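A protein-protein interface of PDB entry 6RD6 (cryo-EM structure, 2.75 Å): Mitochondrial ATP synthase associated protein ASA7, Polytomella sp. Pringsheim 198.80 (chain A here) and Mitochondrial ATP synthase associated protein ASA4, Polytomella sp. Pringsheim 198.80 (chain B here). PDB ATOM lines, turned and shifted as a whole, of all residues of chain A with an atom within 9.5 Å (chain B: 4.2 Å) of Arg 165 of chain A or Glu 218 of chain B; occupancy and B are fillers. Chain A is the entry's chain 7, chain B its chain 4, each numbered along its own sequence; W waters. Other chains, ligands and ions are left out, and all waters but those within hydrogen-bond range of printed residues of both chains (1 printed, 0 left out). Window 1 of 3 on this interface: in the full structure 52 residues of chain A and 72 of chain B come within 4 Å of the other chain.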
ATOM      1  N   LEU A  85      -8.930  -8.013  11.975  1.00  0.00           N
ATOM      2  CA  LEU A  85      -8.424  -8.779  10.843  1.00  0.00           C
ATOM      3  C   LEU A  85      -9.211 -10.070  10.650  1.00  0.00           C
ATOM      4  O   LEU A  85      -9.627 -10.401   9.529  1.00  0.00           O
ATOM      5  CB  LEU A  85      -6.944  -9.069  11.074  1.00  0.00           C
ATOM      6  CG  LEU A  85      -6.257 -10.124  10.226  1.00  0.00           C
ATOM      7  CD1 LEU A  85      -6.173  -9.635   8.821  1.00  0.00           C
ATOM      8  CD2 LEU A  85      -4.886 -10.413  10.776  1.00  0.00           C
ATOM      9  N   ILE A  89     -11.729 -11.179   7.494  1.00  0.00           N
ATOM     10  CA  ILE A  89     -11.609 -12.439   6.763  1.00  0.00           C
ATOM     11  C   ILE A  89     -12.896 -13.253   6.871  1.00  0.00           C
ATOM     12  O   ILE A  89     -13.387 -13.798   5.873  1.00  0.00           O
ATOM     13  CB  ILE A  89     -10.383 -13.225   7.263  1.00  0.00           C
ATOM     14  CG1 ILE A  89      -9.112 -12.430   6.988  1.00  0.00           C
ATOM     15  CG2 ILE A  89     -10.293 -14.578   6.590  1.00  0.00           C
ATOM     16  CD1 ILE A  89      -7.886 -13.024   7.602  1.00  0.00           C
ATOM     17  N   VAL A 157      -6.576 -18.566   7.733  1.00  0.00           N
ATOM     18  CA  VAL A 157      -6.020 -17.580   6.810  1.00  0.00           C
ATOM     19  C   VAL A 157      -5.092 -16.621   7.546  1.00  0.00           C
ATOM     20  O   VAL A 157      -4.087 -16.161   6.994  1.00  0.00           O
ATOM     21  CB  VAL A 157      -7.161 -16.844   6.085  1.00  0.00           C
ATOM     22  CG1 VAL A 157      -6.633 -15.963   4.977  1.00  0.00           C
ATOM     23  CG2 VAL A 157      -8.146 -17.842   5.522  1.00  0.00           C
ATOM     24  N   VAL A 158      -5.404 -16.326   8.805  1.00  0.00           N
ATOM     25  CA  VAL A 158      -4.702 -15.356   9.651  1.00  0.00           C
ATOM     26  C   VAL A 158      -3.202 -15.615   9.837  1.00  0.00           C
ATOM     27  O   VAL A 158      -2.430 -14.672   9.607  1.00  0.00           O
ATOM     28  CB  VAL A 158      -5.414 -15.235  11.012  1.00  0.00           C
ATOM     29  CG1 VAL A 158      -4.567 -14.490  12.025  1.00  0.00           C
ATOM     30  CG2 VAL A 158      -6.741 -14.530  10.843  1.00  0.00           C
ATOM     31  N   PRO A 159      -2.698 -16.851  10.238  1.00  0.00           N
ATOM     32  CA  PRO A 159      -1.277 -16.953  10.621  1.00  0.00           C
ATOM     33  C   PRO A 159      -0.265 -16.717   9.508  1.00  0.00           C
ATOM     34  O   PRO A 159       0.667 -15.929   9.704  1.00  0.00           O
ATOM     35  CB  PRO A 159      -1.163 -18.389  11.151  1.00  0.00           C
ATOM     36  CG  PRO A 159      -2.526 -18.780  11.482  1.00  0.00           C
ATOM     37  CD  PRO A 159      -3.341 -18.166  10.418  1.00  0.00           C
ATOM     38  N   ASN A 160      -0.458 -17.366   8.353  1.00  0.00           N
ATOM     39  CA  ASN A 160       0.466 -17.224   7.228  1.00  0.00           C
ATOM     40  C   ASN A 160       0.544 -15.782   6.752  1.00  0.00           C
ATOM     41  O   ASN A 160       1.642 -15.254   6.532  1.00  0.00           O
ATOM     42  CB  ASN A 160       0.044 -18.134   6.076  1.00  0.00           C
ATOM     43  CG  ASN A 160       0.644 -19.515   6.175  1.00  0.00           C
ATOM     44  OD1 ASN A 160       1.695 -19.703   6.783  1.00  0.00           O
ATOM     45  ND2 ASN A 160      -0.009 -20.489   5.558  1.00  0.00           N
ATOM     46  N   TYR A 161      -0.619 -15.129   6.625  1.00  0.00           N
ATOM     47  CA  TYR A 161      -0.679 -13.704   6.315  1.00  0.00           C
ATOM     48  C   TYR A 161       0.079 -12.883   7.345  1.00  0.00           C
ATOM     49  O   TYR A 161       0.833 -11.971   6.984  1.00  0.00           O
ATOM     50  CB  TYR A 161      -2.135 -13.243   6.246  1.00  0.00           C
ATOM     51  CG  TYR A 161      -2.300 -11.741   6.285  1.00  0.00           C
ATOM     52  CD1 TYR A 161      -2.735 -11.094   7.437  1.00  0.00           C
ATOM     53  CD2 TYR A 161      -2.024 -10.969   5.168  1.00  0.00           C
ATOM     54  CE1 TYR A 161      -2.861  -9.732   7.475  1.00  0.00           C
ATOM     55  CE2 TYR A 161      -2.166  -9.603   5.199  1.00  0.00           C
ATOM     56  CZ  TYR A 161      -2.591  -8.995   6.354  1.00  0.00           C
ATOM     57  OH  TYR A 161      -2.734  -7.634   6.396  1.00  0.00           O
ATOM     58  N   ALA A 162      -0.075 -13.227   8.628  1.00  0.00           N
ATOM     59  CA  ALA A 162       0.634 -12.507   9.675  1.00  0.00           C
ATOM     60  C   ALA A 162       2.131 -12.747   9.576  1.00  0.00           C
ATOM     61  O   ALA A 162       2.930 -11.847   9.863  1.00  0.00           O
ATOM     62  CB  ALA A 162       0.105 -12.920  11.045  1.00  0.00           C
ATOM     63  N   ALA A 163       2.530 -13.927   9.092  1.00  0.00           N
ATOM     64  CA  ALA A 163       3.949 -14.194   8.901  1.00  0.00           C
ATOM     65  C   ALA A 163       4.495 -13.398   7.728  1.00  0.00           C
ATOM     66  O   ALA A 163       5.699 -13.131   7.655  1.00  0.00           O
ATOM     67  CB  ALA A 163       4.181 -15.688   8.699  1.00  0.00           C
ATOM     68  N   ARG A 164       3.624 -12.995   6.802  1.00  0.00           N
ATOM     69  CA  ARG A 164       4.065 -12.108   5.737  1.00  0.00           C
ATOM     70  C   ARG A 164       4.193 -10.683   6.243  1.00  0.00           C
ATOM     71  O   ARG A 164       4.901  -9.866   5.646  1.00  0.00           O
ATOM     72  CB  ARG A 164       3.096 -12.168   4.562  1.00  0.00           C
ATOM     73  CG  ARG A 164       3.154 -13.450   3.779  1.00  0.00           C
ATOM     74  CD  ARG A 164       2.341 -13.326   2.516  1.00  0.00           C
ATOM     75  NE  ARG A 164       2.743 -12.169   1.727  1.00  0.00           N
ATOM     76  CZ  ARG A 164       3.682 -12.197   0.788  1.00  0.00           C
ATOM     77  NH1 ARG A 164       3.981 -11.098   0.117  1.00  0.00           N
ATOM     78  NH2 ARG A 164       4.318 -13.326   0.521  1.00  0.00           N
ATOM     79  N   ARG A 165       3.509 -10.363   7.342  1.00  0.00           N
ATOM     80  CA  ARG A 165       3.533  -8.992   7.836  1.00  0.00           C
ATOM     81  C   ARG A 165       4.686  -8.780   8.800  1.00  0.00           C
ATOM     82  O   ARG A 165       5.107  -7.644   9.036  1.00  0.00           O
ATOM     83  CB  ARG A 165       2.208  -8.654   8.502  1.00  0.00           C
ATOM     84  CG  ARG A 165       1.020  -8.569   7.568  1.00  0.00           C
ATOM     85  CD  ARG A 165       1.236  -7.563   6.461  1.00  0.00           C
ATOM     86  NE  ARG A 165       1.515  -8.241   5.204  1.00  0.00           N
ATOM     87  CZ  ARG A 165       1.923  -7.634   4.101  1.00  0.00           C
ATOM     88  NH1 ARG A 165       2.164  -8.339   3.008  1.00  0.00           N
ATOM     89  NH2 ARG A 165       2.086  -6.322   4.088  1.00  0.00           N
ATOM     90  N   ARG A 166       5.215  -9.864   9.364  1.00  0.00           N
ATOM     91  CA  ARG A 166       6.425  -9.799  10.169  1.00  0.00           C
ATOM     92  C   ARG A 166       7.658  -9.872   9.284  1.00  0.00           C
ATOM     93  O   ARG A 166       8.513 -10.739   9.474  1.00  0.00           O
ATOM     94  CB  ARG A 166       6.459 -10.928  11.191  1.00  0.00           C
ATOM     95  CG  ARG A 166       5.491 -10.766  12.325  1.00  0.00           C
ATOM     96  CD  ARG A 166       5.784 -11.774  13.405  1.00  0.00           C
ATOM     97  NE  ARG A 166       5.722 -13.148  12.918  1.00  0.00           N
ATOM     98  CZ  ARG A 166       4.614 -13.877  12.880  1.00  0.00           C
ATOM     99  NH1 ARG A 166       4.651 -15.117  12.424  1.00  0.00           N
ATOM    100  NH2 ARG A 166       3.468 -13.368  13.300  1.00  0.00           N
ATOM    101  N   SER A 167       7.760  -8.969   8.323  1.00  0.00           N
ATOM    102  CA  SER A 167       8.901  -8.903   7.434  1.00  0.00           C
ATOM    103  C   SER A 167      10.037  -8.191   8.144  1.00  0.00           C
ATOM    104  O   SER A 167       9.808  -7.291   8.955  1.00  0.00           O
ATOM    105  CB  SER A 167       8.543  -8.174   6.141  1.00  0.00           C
ATOM    106  OG  SER A 167       9.657  -8.076   5.277  1.00  0.00           O
ATOM    107  N   THR A 168      11.265  -8.606   7.842  1.00  0.00           N
ATOM    108  CA  THR A 168      12.421  -7.952   8.434  1.00  0.00           C
ATOM    109  C   THR A 168      12.701  -6.602   7.792  1.00  0.00           C
ATOM    110  O   THR A 168      13.484  -5.821   8.337  1.00  0.00           O
ATOM    111  CB  THR A 168      13.644  -8.857   8.323  1.00  0.00           C
ATOM    112  OG1 THR A 168      14.060  -8.936   6.957  1.00  0.00           O
ATOM    113  CG2 THR A 168      13.308 -10.246   8.821  1.00  0.00           C
ATOM    114  N   VAL A 169      12.078  -6.308   6.652  1.00  0.00           N
ATOM    115  CA  VAL A 169      12.210  -4.999   6.030  1.00  0.00           C
ATOM    116  C   VAL A 169      11.133  -4.068   6.568  1.00  0.00           C
ATOM    117  O   VAL A 169      11.438  -3.129   7.303  1.00  0.00           O
ATOM    118  CB  VAL A 169      12.131  -5.102   4.499  1.00  0.00           C
ATOM    119  CG1 VAL A 169      12.231  -3.732   3.879  1.00  0.00           C
ATOM    120  CG2 VAL A 169      13.224  -6.003   3.976  1.00  0.00           C
ATOM    121  N   HIS A 170       9.867  -4.354   6.274  1.00  0.00           N
ATOM    122  CA  HIS A 170       8.774  -3.449   6.604  1.00  0.00           C
ATOM    123  C   HIS A 170       7.470  -4.222   6.499  1.00  0.00           C
ATOM    124  O   HIS A 170       7.373  -5.141   5.682  1.00  0.00           O
ATOM    125  CB  HIS A 170       8.757  -2.236   5.658  1.00  0.00           C
ATOM    126  CG  HIS A 170       7.933  -1.088   6.152  1.00  0.00           C
ATOM    127  ND1 HIS A 170       8.465  -0.040   6.866  1.00  0.00           N
ATOM    128  CD2 HIS A 170       6.612  -0.821   6.029  1.00  0.00           C
ATOM    129  CE1 HIS A 170       7.506   0.814   7.172  1.00  0.00           C
ATOM    130  NE2 HIS A 170       6.372   0.364   6.674  1.00  0.00           N
ATOM    131  N   PRO A 171       6.463  -3.895   7.317  1.00  0.00           N
ATOM    132  CA  PRO A 171       5.151  -4.552   7.169  1.00  0.00           C
ATOM    133  C   PRO A 171       4.453  -4.279   5.848  1.00  0.00           C
ATOM    134  O   PRO A 171       3.638  -5.096   5.411  1.00  0.00           O
ATOM    135  CB  PRO A 171       4.339  -3.978   8.336  1.00  0.00           C
ATOM    136  CG  PRO A 171       5.315  -3.488   9.289  1.00  0.00           C
ATOM    137  CD  PRO A 171       6.582  -3.176   8.596  1.00  0.00           C
ATOM    138  N   ALA A 172       4.741  -3.154   5.203  1.00  0.00           N
ATOM    139  CA  ALA A 172       4.057  -2.728   3.993  1.00  0.00           C
ATOM    140  C   ALA A 172       4.923  -2.831   2.749  1.00  0.00           C
ATOM    141  O   ALA A 172       4.569  -2.256   1.716  1.00  0.00           O
ATOM    142  CB  ALA A 172       3.569  -1.291   4.148  1.00  0.00           C
ATOM    143  N   ILE A 173       6.052  -3.537   2.816  1.00  0.00           N
ATOM    144  CA  ILE A 173       6.912  -3.630   1.645  1.00  0.00           C
ATOM    145  C   ILE A 173       6.315  -4.632   0.666  1.00  0.00           C
ATOM    146  O   ILE A 173       5.659  -5.608   1.055  1.00  0.00           O
ATOM    147  CB  ILE A 173       8.356  -3.972   2.059  1.00  0.00           C
ATOM    148  CG1 ILE A 173       9.332  -3.727   0.909  1.00  0.00           C
ATOM    149  CG2 ILE A 173       8.489  -5.397   2.566  1.00  0.00           C
ATOM    150  CD1 ILE A 173       9.401  -2.302   0.478  1.00  0.00           C
ATOM    151  N   GLY A 174       6.473  -4.347  -0.626  1.00  0.00           N
ATOM    152  CA  GLY A 174       5.973  -5.216  -1.663  1.00  0.00           C
ATOM    153  C   GLY A 174       7.016  -5.391  -2.752  1.00  0.00           C
ATOM    154  O   GLY A 174       8.181  -5.037  -2.584  1.00  0.00           O
ATOM    155  N   SER A 175       6.569  -5.950  -3.874  1.00  0.00           N
ATOM    156  CA  SER A 175       7.488  -6.198  -4.976  1.00  0.00           C
ATOM    157  C   SER A 175       7.787  -4.921  -5.747  1.00  0.00           C
ATOM    158  O   SER A 175       8.928  -4.698  -6.156  1.00  0.00           O
ATOM    159  CB  SER A 175       6.919  -7.262  -5.907  1.00  0.00           C
ATOM    160  OG  SER A 175       6.830  -8.510  -5.249  1.00  0.00           O
ATOM    161  N   VAL B  63       4.482  -4.671  15.737  1.00  0.00           N
ATOM    162  CA  VAL B  63       3.791  -4.952  14.479  1.00  0.00           C
ATOM    163  C   VAL B  63       2.721  -6.020  14.660  1.00  0.00           C
ATOM    164  O   VAL B  63       1.601  -5.876  14.154  1.00  0.00           O
ATOM    165  CB  VAL B  63       4.813  -5.340  13.392  1.00  0.00           C
ATOM    166  CG1 VAL B  63       4.150  -5.995  12.201  1.00  0.00           C
ATOM    167  CG2 VAL B  63       5.510  -4.113  12.903  1.00  0.00           C
ATOM    168  N   VAL B  67      -1.093  -5.576  13.317  1.00  0.00           N
ATOM    169  CA  VAL B  67      -1.544  -6.209  12.082  1.00  0.00           C
ATOM    170  C   VAL B  67      -2.934  -6.796  12.273  1.00  0.00           C
ATOM    171  O   VAL B  67      -3.799  -6.695  11.394  1.00  0.00           O
ATOM    172  CB  VAL B  67      -0.515  -7.265  11.645  1.00  0.00           C
ATOM    173  CG1 VAL B  67      -1.101  -8.289  10.688  1.00  0.00           C
ATOM    174  CG2 VAL B  67       0.646  -6.584  11.014  1.00  0.00           C
ATOM    175  N   LEU B  89      -0.884   0.136   7.283  1.00  0.00           N
ATOM    176  CA  LEU B  89       0.378  -0.592   7.374  1.00  0.00           C
ATOM    177  C   LEU B  89       1.569   0.356   7.446  1.00  0.00           C
ATOM    178  O   LEU B  89       2.549   0.080   8.146  1.00  0.00           O
ATOM    179  CB  LEU B  89       0.518  -1.539   6.189  1.00  0.00           C
ATOM    180  CG  LEU B  89      -0.336  -2.800   6.189  1.00  0.00           C
ATOM    181  CD1 LEU B  89      -0.038  -3.608   4.954  1.00  0.00           C
ATOM    182  CD2 LEU B  89      -0.082  -3.610   7.433  1.00  0.00           C
ATOM    183  N   ASP B 214       0.952  -3.307  -4.499  1.00  0.00           N
ATOM    184  CA  ASP B 214       1.397  -4.386  -3.619  1.00  0.00           C
ATOM    185  C   ASP B 214       0.328  -4.770  -2.602  1.00  0.00           C
ATOM    186  O   ASP B 214       0.122  -5.961  -2.327  1.00  0.00           O
ATOM    187  CB  ASP B 214       2.688  -4.006  -2.901  1.00  0.00           C
ATOM    188  CG  ASP B 214       3.770  -3.554  -3.847  1.00  0.00           C
ATOM    189  OD1 ASP B 214       3.984  -4.230  -4.874  1.00  0.00           O
ATOM    190  OD2 ASP B 214       4.442  -2.550  -3.541  1.00  0.00           O
ATOM    191  N   ALA B 215      -0.372  -3.779  -2.039  1.00  0.00           N
ATOM    192  CA  ALA B 215      -1.437  -4.081  -1.091  1.00  0.00           C
ATOM    193  C   ALA B 215      -2.619  -4.751  -1.779  1.00  0.00           C
ATOM    194  O   ALA B 215      -3.237  -5.658  -1.214  1.00  0.00           O
ATOM    195  CB  ALA B 215      -1.875  -2.806  -0.376  1.00  0.00           C
ATOM    196  N   ALA B 216      -2.919  -4.351  -3.018  1.00  0.00           N
ATOM    197  CA  ALA B 216      -3.983  -5.000  -3.773  1.00  0.00           C
ATOM    198  C   ALA B 216      -3.601  -6.421  -4.157  1.00  0.00           C
ATOM    199  O   ALA B 216      -4.461  -7.305  -4.197  1.00  0.00           O
ATOM    200  CB  ALA B 216      -4.318  -4.177  -5.014  1.00  0.00           C
ATOM    201  N   ALA B 217      -2.314  -6.668  -4.414  1.00  0.00           N
ATOM    202  CA  ALA B 217      -1.861  -8.028  -4.686  1.00  0.00           C
ATOM    203  C   ALA B 217      -1.968  -8.911  -3.450  1.00  0.00           C
ATOM    204  O   ALA B 217      -2.360 -10.081  -3.548  1.00  0.00           O
ATOM    205  CB  ALA B 217      -0.426  -8.005  -5.202  1.00  0.00           C
ATOM    206  N   GLU B 218      -1.639  -8.360  -2.276  1.00  0.00           N
ATOM    207  CA  GLU B 218      -1.787  -9.110  -1.029  1.00  0.00           C
ATOM    208  C   GLU B 218      -3.252  -9.408  -0.729  1.00  0.00           C
ATOM    209  O   GLU B 218      -3.595 -10.510  -0.277  1.00  0.00           O
ATOM    210  CB  GLU B 218      -1.150  -8.330   0.119  1.00  0.00           C
ATOM    211  CG  GLU B 218      -1.015  -9.110   1.406  1.00  0.00           C
ATOM    212  CD  GLU B 218       0.086 -10.148   1.347  1.00  0.00           C
ATOM    213  OE1 GLU B 218      -0.211 -11.347   1.539  1.00  0.00           O
ATOM    214  OE2 GLU B 218       1.250  -9.765   1.108  1.00  0.00           O
ATOM    215  N   VAL B 219      -4.132  -8.443  -1.006  1.00  0.00           N
ATOM    216  CA  VAL B 219      -5.565  -8.636  -0.806  1.00  0.00           C
ATOM    217  C   VAL B 219      -6.115  -9.674  -1.780  1.00  0.00           C
ATOM    218  O   VAL B 219      -6.935 -10.514  -1.400  1.00  0.00           O
ATOM    219  CB  VAL B 219      -6.285  -7.277  -0.919  1.00  0.00           C
ATOM    220  CG1 VAL B 219      -7.782  -7.428  -1.107  1.00  0.00           C
ATOM    221  CG2 VAL B 219      -6.014  -6.468   0.312  1.00  0.00           C
ATOM    222  N   LYS B 220      -5.643  -9.666  -3.030  1.00  0.00           N
ATOM    223  CA  LYS B 220      -6.086 -10.663  -4.004  1.00  0.00           C
ATOM    224  C   LYS B 220      -5.600 -12.059  -3.636  1.00  0.00           C
ATOM    225  O   LYS B 220      -6.317 -13.044  -3.847  1.00  0.00           O
ATOM    226  CB  LYS B 220      -5.603 -10.292  -5.404  1.00  0.00           C
ATOM    227  CG  LYS B 220      -6.393  -9.184  -6.073  1.00  0.00           C
ATOM    228  CD  LYS B 220      -7.875  -9.494  -6.111  1.00  0.00           C
ATOM    229  CE  LYS B 220      -8.650  -8.363  -6.758  1.00  0.00           C
ATOM    230  NZ  LYS B 220     -10.099  -8.677  -6.874  1.00  0.00           N
ATOM    231  N   ALA B 221      -4.397 -12.162  -3.067  1.00  0.00           N
ATOM    232  CA  ALA B 221      -3.905 -13.460  -2.615  1.00  0.00           C
ATOM    233  C   ALA B 221      -4.716 -13.983  -1.438  1.00  0.00           C
ATOM    234  O   ALA B 221      -5.033 -15.177  -1.380  1.00  0.00           O
ATOM    235  CB  ALA B 221      -2.429 -13.364  -2.245  1.00  0.00           C
ATOM    236  N   ILE B 222      -5.075 -13.103  -0.498  1.00  0.00           N
ATOM    237  CA  ILE B 222      -5.887 -13.521   0.644  1.00  0.00           C
ATOM    238  C   ILE B 222      -7.298 -13.891   0.195  1.00  0.00           C
ATOM    239  O   ILE B 222      -7.885 -14.864   0.687  1.00  0.00           O
ATOM    240  CB  ILE B 222      -5.879 -12.420   1.723  1.00  0.00           C
ATOM    241  CG1 ILE B 222      -4.508 -12.350   2.383  1.00  0.00           C
ATOM    242  CG2 ILE B 222      -6.919 -12.668   2.803  1.00  0.00           C
ATOM    243  CD1 ILE B 222      -4.124 -13.621   3.092  1.00  0.00           C
HETATM  244  O   HOH W   1      -4.002  -6.592   8.640  1.00  0.00           O
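Water W1 bridges O of Val 67 of chain B (2.8 Å) and OH of Tyr 161 of chain A (2.8 Å).
Among the printed residues, merely in contact across the chains: Gly 174 of chain A with Asp 214 of chain B (3.5 Å), Arg 165 of chain A with Leu 89 of chain B (3.6 Å), Arg 165 of chain A with Val 67 of chain B (3.6 Å), Pro 171 of chain A with Val 63 of chain B (3.7 Å), Ala 172 of chain A with Leu 89 of chain B (3.7 Å), Arg 165 of chain A with Val 63 of chain B (3.7 Å), Tyr 161 of chain A with Ile 222 of chain B (3.7 Å), Val 157 of chain A with Ile 222 of chain B (3.9 Å), Leu 85 of chain A with Val 67 of chain B (3.9 Å), Tyr 161 of chain A with Val 67 of chain B (3.9 Å), Pro 171 of chain A with Leu 89 of chain B (3.99 Å) and Tyr 161 of chain A with Glu 218 of chain B (3.99 Å).
Of the 12 printed residues of chain B, 6 touch a printed residue of chain A. Hydrophobic or aromatic side chains of chain B within 4 Å of the printed part of chain A: Val 63, Val 67, Leu 89 and Ile 222. Of the 21 printed residues of chain A, 9 touch a printed residue of chain B. Hydrophobic or aromatic side chains of chain A within 4 Å of the printed part of chain B: Leu 85, Val 157, Tyr 161, Pro 171 and Ala 172. Among the printed residues, 15 pairs touch across the chains.
Arg 165 of chain A touches just these residues of chain B: Val 63 (3.7 Å), Val 67 (3.6 Å), Leu 89 (3.6 Å) and Glu 218 (2.5 Å). No residue of chain A comes within 4 Å of Ala 217 of chain B. No residue of chain A comes within 4 Å of Val 219 of chain B. No residue of chain A comes within 4 Å of Ala 221 of chain B. Of the printed residues of chain A, Ile 222 of chain B touches Val 157 and Tyr 161. Of the printed residues of chain B, Arg 164 of chain A touches Glu 218. Of the printed residues of chain B, Val 157 of chain A touches Ile 222 (3.9 Å). Of the printed residues of chain A, Leu 89 of chain B touches Arg 165 (3.6 Å), Pro 171 (3.99 Å) and Ala 172 (3.7 Å). Ser 167 of chain A touches none of the printed residues of chain B. Ile 173 of chain A touches none of the printed residues of chain B.
The side-chain carboxylate of Asp 214 of chain B lies within hydrogen-bond range of the backbone NH of Ser 175 of chain A (3.3 Å). The side-chain carboxylate of Glu 218 of chain B is in salt-bridge range of the guanidinium group of Arg 164 of chain A (2.9 Å). The guanidinium group (NH1) of Arg 165 of chain A lies within salt-bridge range of the side-chain carboxylate (OE2) of Glu 218 of chain B (2.5 Å).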
